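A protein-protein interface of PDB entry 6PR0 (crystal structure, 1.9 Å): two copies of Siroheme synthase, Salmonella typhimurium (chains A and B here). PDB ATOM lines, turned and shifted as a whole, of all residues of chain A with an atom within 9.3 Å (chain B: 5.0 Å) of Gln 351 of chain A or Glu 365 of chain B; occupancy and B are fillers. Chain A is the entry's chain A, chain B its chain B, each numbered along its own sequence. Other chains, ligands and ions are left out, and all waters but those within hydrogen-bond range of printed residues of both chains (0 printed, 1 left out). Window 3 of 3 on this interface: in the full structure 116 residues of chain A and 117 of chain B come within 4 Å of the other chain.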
ATOM      1  N   LEU A 344     -11.246 -15.067 -31.427  1.00  0.00           N
ATOM      2  CA  LEU A 344     -11.691 -16.164 -30.573  1.00  0.00           C
ATOM      3  C   LEU A 344     -10.502 -16.874 -29.942  1.00  0.00           C
ATOM      4  O   LEU A 344     -10.630 -17.470 -28.860  1.00  0.00           O
ATOM      5  CB  LEU A 344     -12.544 -17.157 -31.383  1.00  0.00           C
ATOM      6  CG  LEU A 344     -13.867 -16.630 -31.955  1.00  0.00           C
ATOM      7  CD1 LEU A 344     -14.643 -17.701 -32.738  1.00  0.00           C
ATOM      8  CD2 LEU A 344     -14.749 -16.023 -30.859  1.00  0.00           C
ATOM      9  N   THR A 345      -9.355 -16.857 -30.612  1.00  0.00           N
ATOM     10  CA  THR A 345      -8.113 -17.349 -30.028  1.00  0.00           C
ATOM     11  C   THR A 345      -7.035 -16.296 -30.240  1.00  0.00           C
ATOM     12  O   THR A 345      -7.098 -15.513 -31.194  1.00  0.00           O
ATOM     13  CB  THR A 345      -7.661 -18.689 -30.656  1.00  0.00           C
ATOM     14  OG1 THR A 345      -7.264 -18.483 -32.025  1.00  0.00           O
ATOM     15  CG2 THR A 345      -8.792 -19.688 -30.644  1.00  0.00           C
ATOM     16  N   HIS A 346      -6.043 -16.286 -29.349  1.00  0.00           N
ATOM     17  CA  HIS A 346      -4.939 -15.332 -29.448  1.00  0.00           C
ATOM     18  C   HIS A 346      -3.843 -15.737 -28.481  1.00  0.00           C
ATOM     19  O   HIS A 346      -4.095 -15.846 -27.275  1.00  0.00           O
ATOM     20  CB  HIS A 346      -5.401 -13.896 -29.146  1.00  0.00           C
ATOM     21  CG  HIS A 346      -4.296 -12.879 -29.218  1.00  0.00           C
ATOM     22  ND1 HIS A 346      -3.798 -12.412 -30.415  1.00  0.00           N
ATOM     23  CD2 HIS A 346      -3.585 -12.250 -28.246  1.00  0.00           C
ATOM     24  CE1 HIS A 346      -2.826 -11.544 -30.184  1.00  0.00           C
ATOM     25  NE2 HIS A 346      -2.679 -11.426 -28.876  1.00  0.00           N
ATOM     26  N   ARG A 347      -2.640 -15.971 -28.994  1.00  0.00           N
ATOM     27  CA  ARG A 347      -1.479 -16.342 -28.182  1.00  0.00           C
ATOM     28  C   ARG A 347      -1.899 -17.467 -27.240  1.00  0.00           C
ATOM     29  O   ARG A 347      -2.580 -18.402 -27.678  1.00  0.00           O
ATOM     30  CB  ARG A 347      -0.938 -15.110 -27.482  1.00  0.00           C
ATOM     31  CG  ARG A 347      -0.335 -14.081 -28.406  1.00  0.00           C
ATOM     32  CD  ARG A 347       0.466 -13.068 -27.612  1.00  0.00           C
ATOM     33  NE  ARG A 347       0.906 -11.959 -28.455  1.00  0.00           N
ATOM     34  CZ  ARG A 347       1.944 -12.019 -29.286  1.00  0.00           C
ATOM     35  NH1 ARG A 347       2.655 -13.136 -29.383  1.00  0.00           N
ATOM     36  NH2 ARG A 347       2.276 -10.963 -30.020  1.00  0.00           N
ATOM     37  N   ASP A 348      -1.550 -17.403 -25.961  1.00  0.00           N
ATOM     38  CA  ASP A 348      -1.902 -18.398 -24.960  1.00  0.00           C
ATOM     39  C   ASP A 348      -3.252 -18.141 -24.304  1.00  0.00           C
ATOM     40  O   ASP A 348      -3.554 -18.797 -23.301  1.00  0.00           O
ATOM     41  CB  ASP A 348      -0.838 -18.436 -23.856  1.00  0.00           C
ATOM     42  CG  ASP A 348       0.570 -18.486 -24.391  1.00  0.00           C
ATOM     43  OD1 ASP A 348       1.275 -17.457 -24.281  1.00  0.00           O
ATOM     44  OD2 ASP A 348       0.979 -19.552 -24.902  1.00  0.00           O
ATOM     45  N   TYR A 349      -4.056 -17.202 -24.831  1.00  0.00           N
ATOM     46  CA  TYR A 349      -5.267 -16.776 -24.127  1.00  0.00           C
ATOM     47  C   TYR A 349      -6.269 -17.913 -24.010  1.00  0.00           C
ATOM     48  O   TYR A 349      -6.883 -18.094 -22.953  1.00  0.00           O
ATOM     49  CB  TYR A 349      -5.929 -15.584 -24.827  1.00  0.00           C
ATOM     50  CG  TYR A 349      -5.293 -14.218 -24.588  1.00  0.00           C
ATOM     51  CD1 TYR A 349      -6.086 -13.101 -24.353  1.00  0.00           C
ATOM     52  CD2 TYR A 349      -3.919 -14.038 -24.645  1.00  0.00           C
ATOM     53  CE1 TYR A 349      -5.533 -11.852 -24.150  1.00  0.00           C
ATOM     54  CE2 TYR A 349      -3.352 -12.784 -24.443  1.00  0.00           C
ATOM     55  CZ  TYR A 349      -4.169 -11.695 -24.200  1.00  0.00           C
ATOM     56  OH  TYR A 349      -3.615 -10.449 -24.000  1.00  0.00           O
ATOM     57  N   ALA A 350      -6.471 -18.679 -25.091  1.00  0.00           N
ATOM     58  CA  ALA A 350      -7.420 -19.786 -25.079  1.00  0.00           C
ATOM     59  C   ALA A 350      -6.813 -21.008 -25.754  1.00  0.00           C
ATOM     60  O   ALA A 350      -6.301 -20.916 -26.872  1.00  0.00           O
ATOM     61  CB  ALA A 350      -8.730 -19.399 -25.775  1.00  0.00           C
ATOM     62  N   GLN A 351      -6.871 -22.148 -25.060  1.00  0.00           N
ATOM     63  CA  GLN A 351      -6.602 -23.441 -25.670  1.00  0.00           C
ATOM     64  C   GLN A 351      -7.800 -23.965 -26.461  1.00  0.00           C
ATOM     65  O   GLN A 351      -7.643 -24.839 -27.320  1.00  0.00           O
ATOM     66  CB  GLN A 351      -6.226 -24.450 -24.587  1.00  0.00           C
ATOM     67  CG  GLN A 351      -4.760 -24.433 -24.196  1.00  0.00           C
ATOM     68  CD  GLN A 351      -4.424 -25.498 -23.170  1.00  0.00           C
ATOM     69  OE1 GLN A 351      -3.891 -26.552 -23.511  1.00  0.00           O
ATOM     70  NE2 GLN A 351      -4.741 -25.228 -21.905  1.00  0.00           N
ATOM     71  N   SER A 352      -8.999 -23.477 -26.176  1.00  0.00           N
ATOM     72  CA  SER A 352     -10.131 -23.894 -26.976  1.00  0.00           C
ATOM     73  C   SER A 352     -11.198 -22.812 -26.982  1.00  0.00           C
ATOM     74  O   SER A 352     -11.248 -21.933 -26.119  1.00  0.00           O
ATOM     75  CB  SER A 352     -10.713 -25.235 -26.495  1.00  0.00           C
ATOM     76  OG  SER A 352     -11.010 -25.237 -25.122  1.00  0.00           O
ATOM     77  N   VAL A 353     -12.023 -22.879 -28.016  1.00  0.00           N
ATOM     78  CA  VAL A 353     -13.230 -22.083 -28.154  1.00  0.00           C
ATOM     79  C   VAL A 353     -14.393 -23.030 -27.904  1.00  0.00           C
ATOM     80  O   VAL A 353     -14.433 -24.125 -28.481  1.00  0.00           O
ATOM     81  CB  VAL A 353     -13.327 -21.467 -29.561  1.00  0.00           C
ATOM     82  CG1 VAL A 353     -14.472 -20.454 -29.646  1.00  0.00           C
ATOM     83  CG2 VAL A 353     -11.980 -20.828 -29.954  1.00  0.00           C
ATOM     84  N   ARG A 354     -15.319 -22.622 -27.054  1.00  0.00           N
ATOM     85  CA  ARG A 354     -16.524 -23.394 -26.772  1.00  0.00           C
ATOM     86  C   ARG A 354     -17.711 -22.643 -27.351  1.00  0.00           C
ATOM     87  O   ARG A 354     -17.966 -21.493 -26.976  1.00  0.00           O
ATOM     88  CB  ARG A 354     -16.730 -23.602 -25.268  1.00  0.00           C
ATOM     89  CG  ARG A 354     -15.487 -23.957 -24.497  1.00  0.00           C
ATOM     90  CD  ARG A 354     -15.284 -25.453 -24.435  1.00  0.00           C
ATOM     91  NE  ARG A 354     -16.464 -26.171 -23.954  1.00  0.00           N
ATOM     92  CZ  ARG A 354     -16.646 -26.560 -22.694  1.00  0.00           C
ATOM     93  NH1 ARG A 354     -15.725 -26.295 -21.775  1.00  0.00           N
ATOM     94  NH2 ARG A 354     -17.747 -27.228 -22.359  1.00  0.00           N
ATOM     95  N   ALA A 373     -13.855 -23.423 -16.671  1.00  0.00           N
ATOM     96  CA  ALA A 373     -12.421 -23.691 -16.698  1.00  0.00           C
ATOM     97  C   ALA A 373     -11.646 -22.558 -17.365  1.00  0.00           C
ATOM     98  O   ALA A 373     -12.155 -21.859 -18.245  1.00  0.00           O
ATOM     99  CB  ALA A 373     -12.143 -25.001 -17.431  1.00  0.00           C
ATOM    100  N   GLU A 374     -10.389 -22.391 -16.945  1.00  0.00           N
ATOM    101  CA  GLU A 374      -9.517 -21.357 -17.489  1.00  0.00           C
ATOM    102  C   GLU A 374      -9.069 -21.691 -18.915  1.00  0.00           C
ATOM    103  O   GLU A 374      -9.150 -22.833 -19.378  1.00  0.00           O
ATOM    104  CB  GLU A 374      -8.276 -21.175 -16.608  1.00  0.00           C
ATOM    105  CG  GLU A 374      -8.563 -20.640 -15.208  1.00  0.00           C
ATOM    106  CD  GLU A 374      -7.311 -20.129 -14.497  1.00  0.00           C
ATOM    107  OE1 GLU A 374      -7.400 -19.103 -13.781  1.00  0.00           O
ATOM    108  OE2 GLU A 374      -6.235 -20.747 -14.663  1.00  0.00           O
ATOM    109  N   LYS A 375      -8.563 -20.659 -19.596  1.00  0.00           N
ATOM    110  CA  LYS A 375      -7.894 -20.781 -20.899  1.00  0.00           C
ATOM    111  C   LYS A 375      -8.881 -21.182 -21.994  1.00  0.00           C
ATOM    112  O   LYS A 375      -8.588 -22.030 -22.840  1.00  0.00           O
ATOM    113  CB  LYS A 375      -6.720 -21.763 -20.849  1.00  0.00           C
ATOM    114  CG  LYS A 375      -5.535 -21.288 -20.004  1.00  0.00           C
ATOM    115  CD  LYS A 375      -4.891 -20.029 -20.584  1.00  0.00           C
ATOM    116  CE  LYS A 375      -3.727 -19.544 -19.723  1.00  0.00           C
ATOM    117  NZ  LYS A 375      -3.056 -18.345 -20.298  1.00  0.00           N
ATOM    118  N   GLN A 376     -10.056 -20.567 -21.987  1.00  0.00           N
ATOM    119  CA  GLN A 376     -10.986 -20.790 -23.080  1.00  0.00           C
ATOM    120  C   GLN A 376     -11.767 -19.523 -23.366  1.00  0.00           C
ATOM    121  O   GLN A 376     -11.832 -18.594 -22.566  1.00  0.00           O
ATOM    122  CB  GLN A 376     -11.938 -21.957 -22.813  1.00  0.00           C
ATOM    123  CG  GLN A 376     -12.398 -22.148 -21.405  1.00  0.00           C
ATOM    124  CD  GLN A 376     -13.129 -23.473 -21.219  1.00  0.00           C
ATOM    125  OE1 GLN A 376     -13.022 -24.374 -22.048  1.00  0.00           O
ATOM    126  NE2 GLN A 376     -13.886 -23.587 -20.138  1.00  0.00           N
ATOM    127  N   THR A 377     -12.308 -19.474 -24.564  1.00  0.00           N
ATOM    128  CA  THR A 377     -13.203 -18.418 -24.970  1.00  0.00           C
ATOM    129  C   THR A 377     -14.575 -19.071 -25.084  1.00  0.00           C
ATOM    130  O   THR A 377     -14.730 -20.024 -25.853  1.00  0.00           O
ATOM    131  CB  THR A 377     -12.737 -17.836 -26.304  1.00  0.00           C
ATOM    132  OG1 THR A 377     -11.406 -17.307 -26.159  1.00  0.00           O
ATOM    133  CG2 THR A 377     -13.705 -16.772 -26.807  1.00  0.00           C
ATOM    134  N   VAL A 444      -9.873 -12.766 -24.271  1.00  0.00           N
ATOM    135  CA  VAL A 444      -9.681 -12.166 -25.591  1.00  0.00           C
ATOM    136  C   VAL A 444     -10.531 -10.927 -25.775  1.00  0.00           C
ATOM    137  O   VAL A 444     -10.244 -10.116 -26.668  1.00  0.00           O
ATOM    138  CB  VAL A 444      -9.999 -13.149 -26.739  1.00  0.00           C
ATOM    139  CG1 VAL A 444      -8.917 -14.242 -26.824  1.00  0.00           C
ATOM    140  CG2 VAL A 444     -11.386 -13.772 -26.533  1.00  0.00           C
ATOM    141  N   PHE B 307      -7.106 -20.118 -34.293  1.00  0.00           N
ATOM    142  CA  PHE B 307      -5.786 -20.757 -34.371  1.00  0.00           C
ATOM    143  C   PHE B 307      -4.996 -20.303 -35.601  1.00  0.00           C
ATOM    144  O   PHE B 307      -4.084 -20.993 -36.065  1.00  0.00           O
ATOM    145  CB  PHE B 307      -5.908 -22.283 -34.322  1.00  0.00           C
ATOM    146  CG  PHE B 307      -6.658 -22.790 -33.109  1.00  0.00           C
ATOM    147  CD1 PHE B 307      -7.833 -23.510 -33.245  1.00  0.00           C
ATOM    148  CD2 PHE B 307      -6.190 -22.518 -31.834  1.00  0.00           C
ATOM    149  CE1 PHE B 307      -8.515 -23.965 -32.129  1.00  0.00           C
ATOM    150  CE2 PHE B 307      -6.872 -22.960 -30.721  1.00  0.00           C
ATOM    151  CZ  PHE B 307      -8.035 -23.688 -30.871  1.00  0.00           C
ATOM    152  N   LEU B 355     -13.633 -26.312 -30.061  1.00  0.00           N
ATOM    153  CA  LEU B 355     -12.556 -26.194 -31.036  1.00  0.00           C
ATOM    154  C   LEU B 355     -11.262 -26.143 -30.239  1.00  0.00           C
ATOM    155  O   LEU B 355     -11.042 -25.175 -29.509  1.00  0.00           O
ATOM    156  CB  LEU B 355     -12.746 -24.936 -31.877  1.00  0.00           C
ATOM    157  CG  LEU B 355     -14.125 -24.735 -32.531  1.00  0.00           C
ATOM    158  CD1 LEU B 355     -14.102 -23.558 -33.476  1.00  0.00           C
ATOM    159  CD2 LEU B 355     -14.558 -25.991 -33.256  1.00  0.00           C
ATOM    160  N   VAL B 356     -10.423 -27.181 -30.356  1.00  0.00           N
ATOM    161  CA  VAL B 356      -9.250 -27.363 -29.494  1.00  0.00           C
ATOM    162  C   VAL B 356      -7.986 -27.495 -30.333  1.00  0.00           C
ATOM    163  O   VAL B 356      -7.982 -28.196 -31.349  1.00  0.00           O
ATOM    164  CB  VAL B 356      -9.361 -28.626 -28.616  1.00  0.00           C
ATOM    165  CG1 VAL B 356      -8.424 -28.525 -27.416  1.00  0.00           C
ATOM    166  CG2 VAL B 356     -10.771 -28.918 -28.231  1.00  0.00           C
ATOM    167  N   THR B 357      -6.887 -26.905 -29.851  1.00  0.00           N
ATOM    168  CA  THR B 357      -5.580 -27.104 -30.474  1.00  0.00           C
ATOM    169  C   THR B 357      -4.847 -28.269 -29.820  1.00  0.00           C
ATOM    170  O   THR B 357      -4.843 -28.411 -28.594  1.00  0.00           O
ATOM    171  CB  THR B 357      -4.710 -25.842 -30.379  1.00  0.00           C
ATOM    172  OG1 THR B 357      -3.420 -26.113 -30.942  1.00  0.00           O
ATOM    173  CG2 THR B 357      -4.521 -25.392 -28.923  1.00  0.00           C
ATOM    174  N   GLY B 364       2.054 -25.059 -20.948  1.00  0.00           N
ATOM    175  CA  GLY B 364       0.673 -25.444 -20.720  1.00  0.00           C
ATOM    176  C   GLY B 364       0.314 -26.790 -21.323  1.00  0.00           C
ATOM    177  O   GLY B 364       1.027 -27.309 -22.186  1.00  0.00           O
ATOM    178  N   GLU B 365      -0.802 -27.359 -20.875  1.00  0.00           N
ATOM    179  CA  GLU B 365      -1.215 -28.670 -21.352  1.00  0.00           C
ATOM    180  C   GLU B 365      -2.734 -28.757 -21.274  1.00  0.00           C
ATOM    181  O   GLU B 365      -3.362 -28.123 -20.423  1.00  0.00           O
ATOM    182  CB  GLU B 365      -0.535 -29.783 -20.534  1.00  0.00           C
ATOM    183  CG  GLU B 365      -0.758 -31.221 -21.000  1.00  0.00           C
ATOM    184  CD  GLU B 365      -1.055 -31.329 -22.485  1.00  0.00           C
ATOM    185  OE1 GLU B 365      -0.168 -31.034 -23.309  1.00  0.00           O
ATOM    186  OE2 GLU B 365      -2.175 -31.741 -22.832  1.00  0.00           O
ATOM    187  N   LEU B 366      -3.311 -29.533 -22.186  1.00  0.00           N
ATOM    188  CA  LEU B 366      -4.759 -29.701 -22.265  1.00  0.00           C
ATOM    189  C   LEU B 366      -5.337 -30.272 -20.969  1.00  0.00           C
ATOM    190  O   LEU B 366      -4.716 -31.111 -20.306  1.00  0.00           O
ATOM    191  CB  LEU B 366      -5.101 -30.629 -23.433  1.00  0.00           C
ATOM    192  CG  LEU B 366      -4.663 -30.152 -24.819  1.00  0.00           C
ATOM    193  CD1 LEU B 366      -4.945 -31.232 -25.835  1.00  0.00           C
ATOM    194  CD2 LEU B 366      -5.373 -28.855 -25.211  1.00  0.00           C
ATOM    195  N   ASP B 367      -6.538 -29.816 -20.611  1.00  0.00           N
ATOM    196  CA  ASP B 367      -7.247 -30.284 -19.415  1.00  0.00           C
ATOM    197  C   ASP B 367      -8.078 -31.510 -19.792  1.00  0.00           C
ATOM    198  O   ASP B 367      -9.204 -31.381 -20.271  1.00  0.00           O
ATOM    199  CB  ASP B 367      -8.122 -29.167 -18.849  1.00  0.00           C
ATOM    200  CG  ASP B 367      -8.673 -29.482 -17.452  1.00  0.00           C
ATOM    201  OD1 ASP B 367      -8.954 -30.663 -17.146  1.00  0.00           O
ATOM    202  OD2 ASP B 367      -8.828 -28.528 -16.656  1.00  0.00           O
ATOM    203  N   TRP B 368      -7.545 -32.708 -19.532  1.00  0.00           N
ATOM    204  CA  TRP B 368      -8.155 -33.923 -20.077  1.00  0.00           C
ATOM    205  C   TRP B 368      -9.498 -34.241 -19.426  1.00  0.00           C
ATOM    206  O   TRP B 368     -10.435 -34.687 -20.102  1.00  0.00           O
ATOM    207  CB  TRP B 368      -7.187 -35.091 -19.929  1.00  0.00           C
ATOM    208  CG  TRP B 368      -6.011 -34.918 -20.803  1.00  0.00           C
ATOM    209  CD1 TRP B 368      -4.716 -34.760 -20.413  1.00  0.00           C
ATOM    210  CD2 TRP B 368      -6.018 -34.840 -22.231  1.00  0.00           C
ATOM    211  NE1 TRP B 368      -3.912 -34.602 -21.511  1.00  0.00           N
ATOM    212  CE2 TRP B 368      -4.686 -34.651 -22.642  1.00  0.00           C
ATOM    213  CE3 TRP B 368      -7.018 -34.934 -23.203  1.00  0.00           C
ATOM    214  CZ2 TRP B 368      -4.327 -34.542 -23.985  1.00  0.00           C
ATOM    215  CZ3 TRP B 368      -6.662 -34.820 -24.541  1.00  0.00           C
ATOM    216  CH2 TRP B 368      -5.329 -34.626 -24.918  1.00  0.00           C
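The backbone NH (N) of Thr 357 of chain B lies within hydrogen-bond range of the backbone carbonyl oxygen (O) of Gln 351 of chain A (3.4 Å).
The backbone carbonyl oxygen (O) of Val 353 of chain A lies within hydrogen-bond range of the backbone NH (N) of Leu 355 of chain B, at 2.8 Å.
OE1 of Gln 351 of chain A lies close to N of Leu 366 of chain B, at 3.3 Å.
The backbone NH (N) of Phe 307 of chain B is in hydrogen-bond range of the side-chain hydroxyl (OG1) of Thr 345 of chain A.
The backbone NH of Gln 351 of chain A lies within hydrogen-bond range of the backbone carbonyl oxygen of Lys 375 of chain A (2.8 Å).
The backbone carbonyl oxygen (O) of Ser 352 of chain A lies within hydrogen-bond range of the backbone NH (N) of Thr 377 of chain A.
Gln 351 of chain A touches Phe 307 of chain B.
Gln 351 of chain A touches Val 356 of chain B (O to CA, 3.7 Å).
Glu 365 of chain B touches Gln 351 of chain A (C to OE1, 3.3 Å).
Ser 352 of chain A touches Leu 355 of chain B (CA to O, 3.0 Å).
Val 356 of chain B touches Ser 352 of chain A (CA to CB, 3.96 Å).
Of chain B, only Phe 307 (3.8 Å), Val 356 (3.7 Å), Thr 357 (3.4 Å), Glu 365 (3.3 Å) and Leu 366 (3.2 Å) come within 4 Å of Gln 351 of chain A.
Of the printed residues of chain A, Glu 365 of chain B touches Gln 351.
No residue of chain A comes within 4 Å of Gly 364 of chain B.
Of chain A, only Gln 351 (3.2 Å) comes within 4 Å of Leu 366 of chain B.
Of the printed residues of chain A, Phe 307 of chain B touches Thr 345 and Gln 351.
Printed residues of chain A within 4 Å of Val 356 of chain B: Gln 351 and Ser 352.
Printed residues of chain B within 4 Å of Val 353 of chain A: Leu 355.
Of the printed residues of chain A, Thr 357 of chain B touches Gln 351 (3.4 Å).
Ala 350 of chain A touches none of the printed residues of chain B.
Tyr 349 of chain A touches none of the printed residues of chain B.
The nearest residue of chain B that does not touch Gln 351 of chain A is Leu 355 of chain B (4.1 Å).
The nearest residue of chain A that does not touch Glu 365 of chain B is Lys 375 of chain A (7.2 Å).
Hydrophobic or aromatic side chains of chain B that line the printed part of chain A: Phe 307, Leu 355, Val 356 and Leu 366.
Among the printed residues, 9 pairs touch across the chains.
No position is printed for both chains.
Of the 9 pairs that touch across the chains among the printed residues, none has its exchanged pair printed and touching as well.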
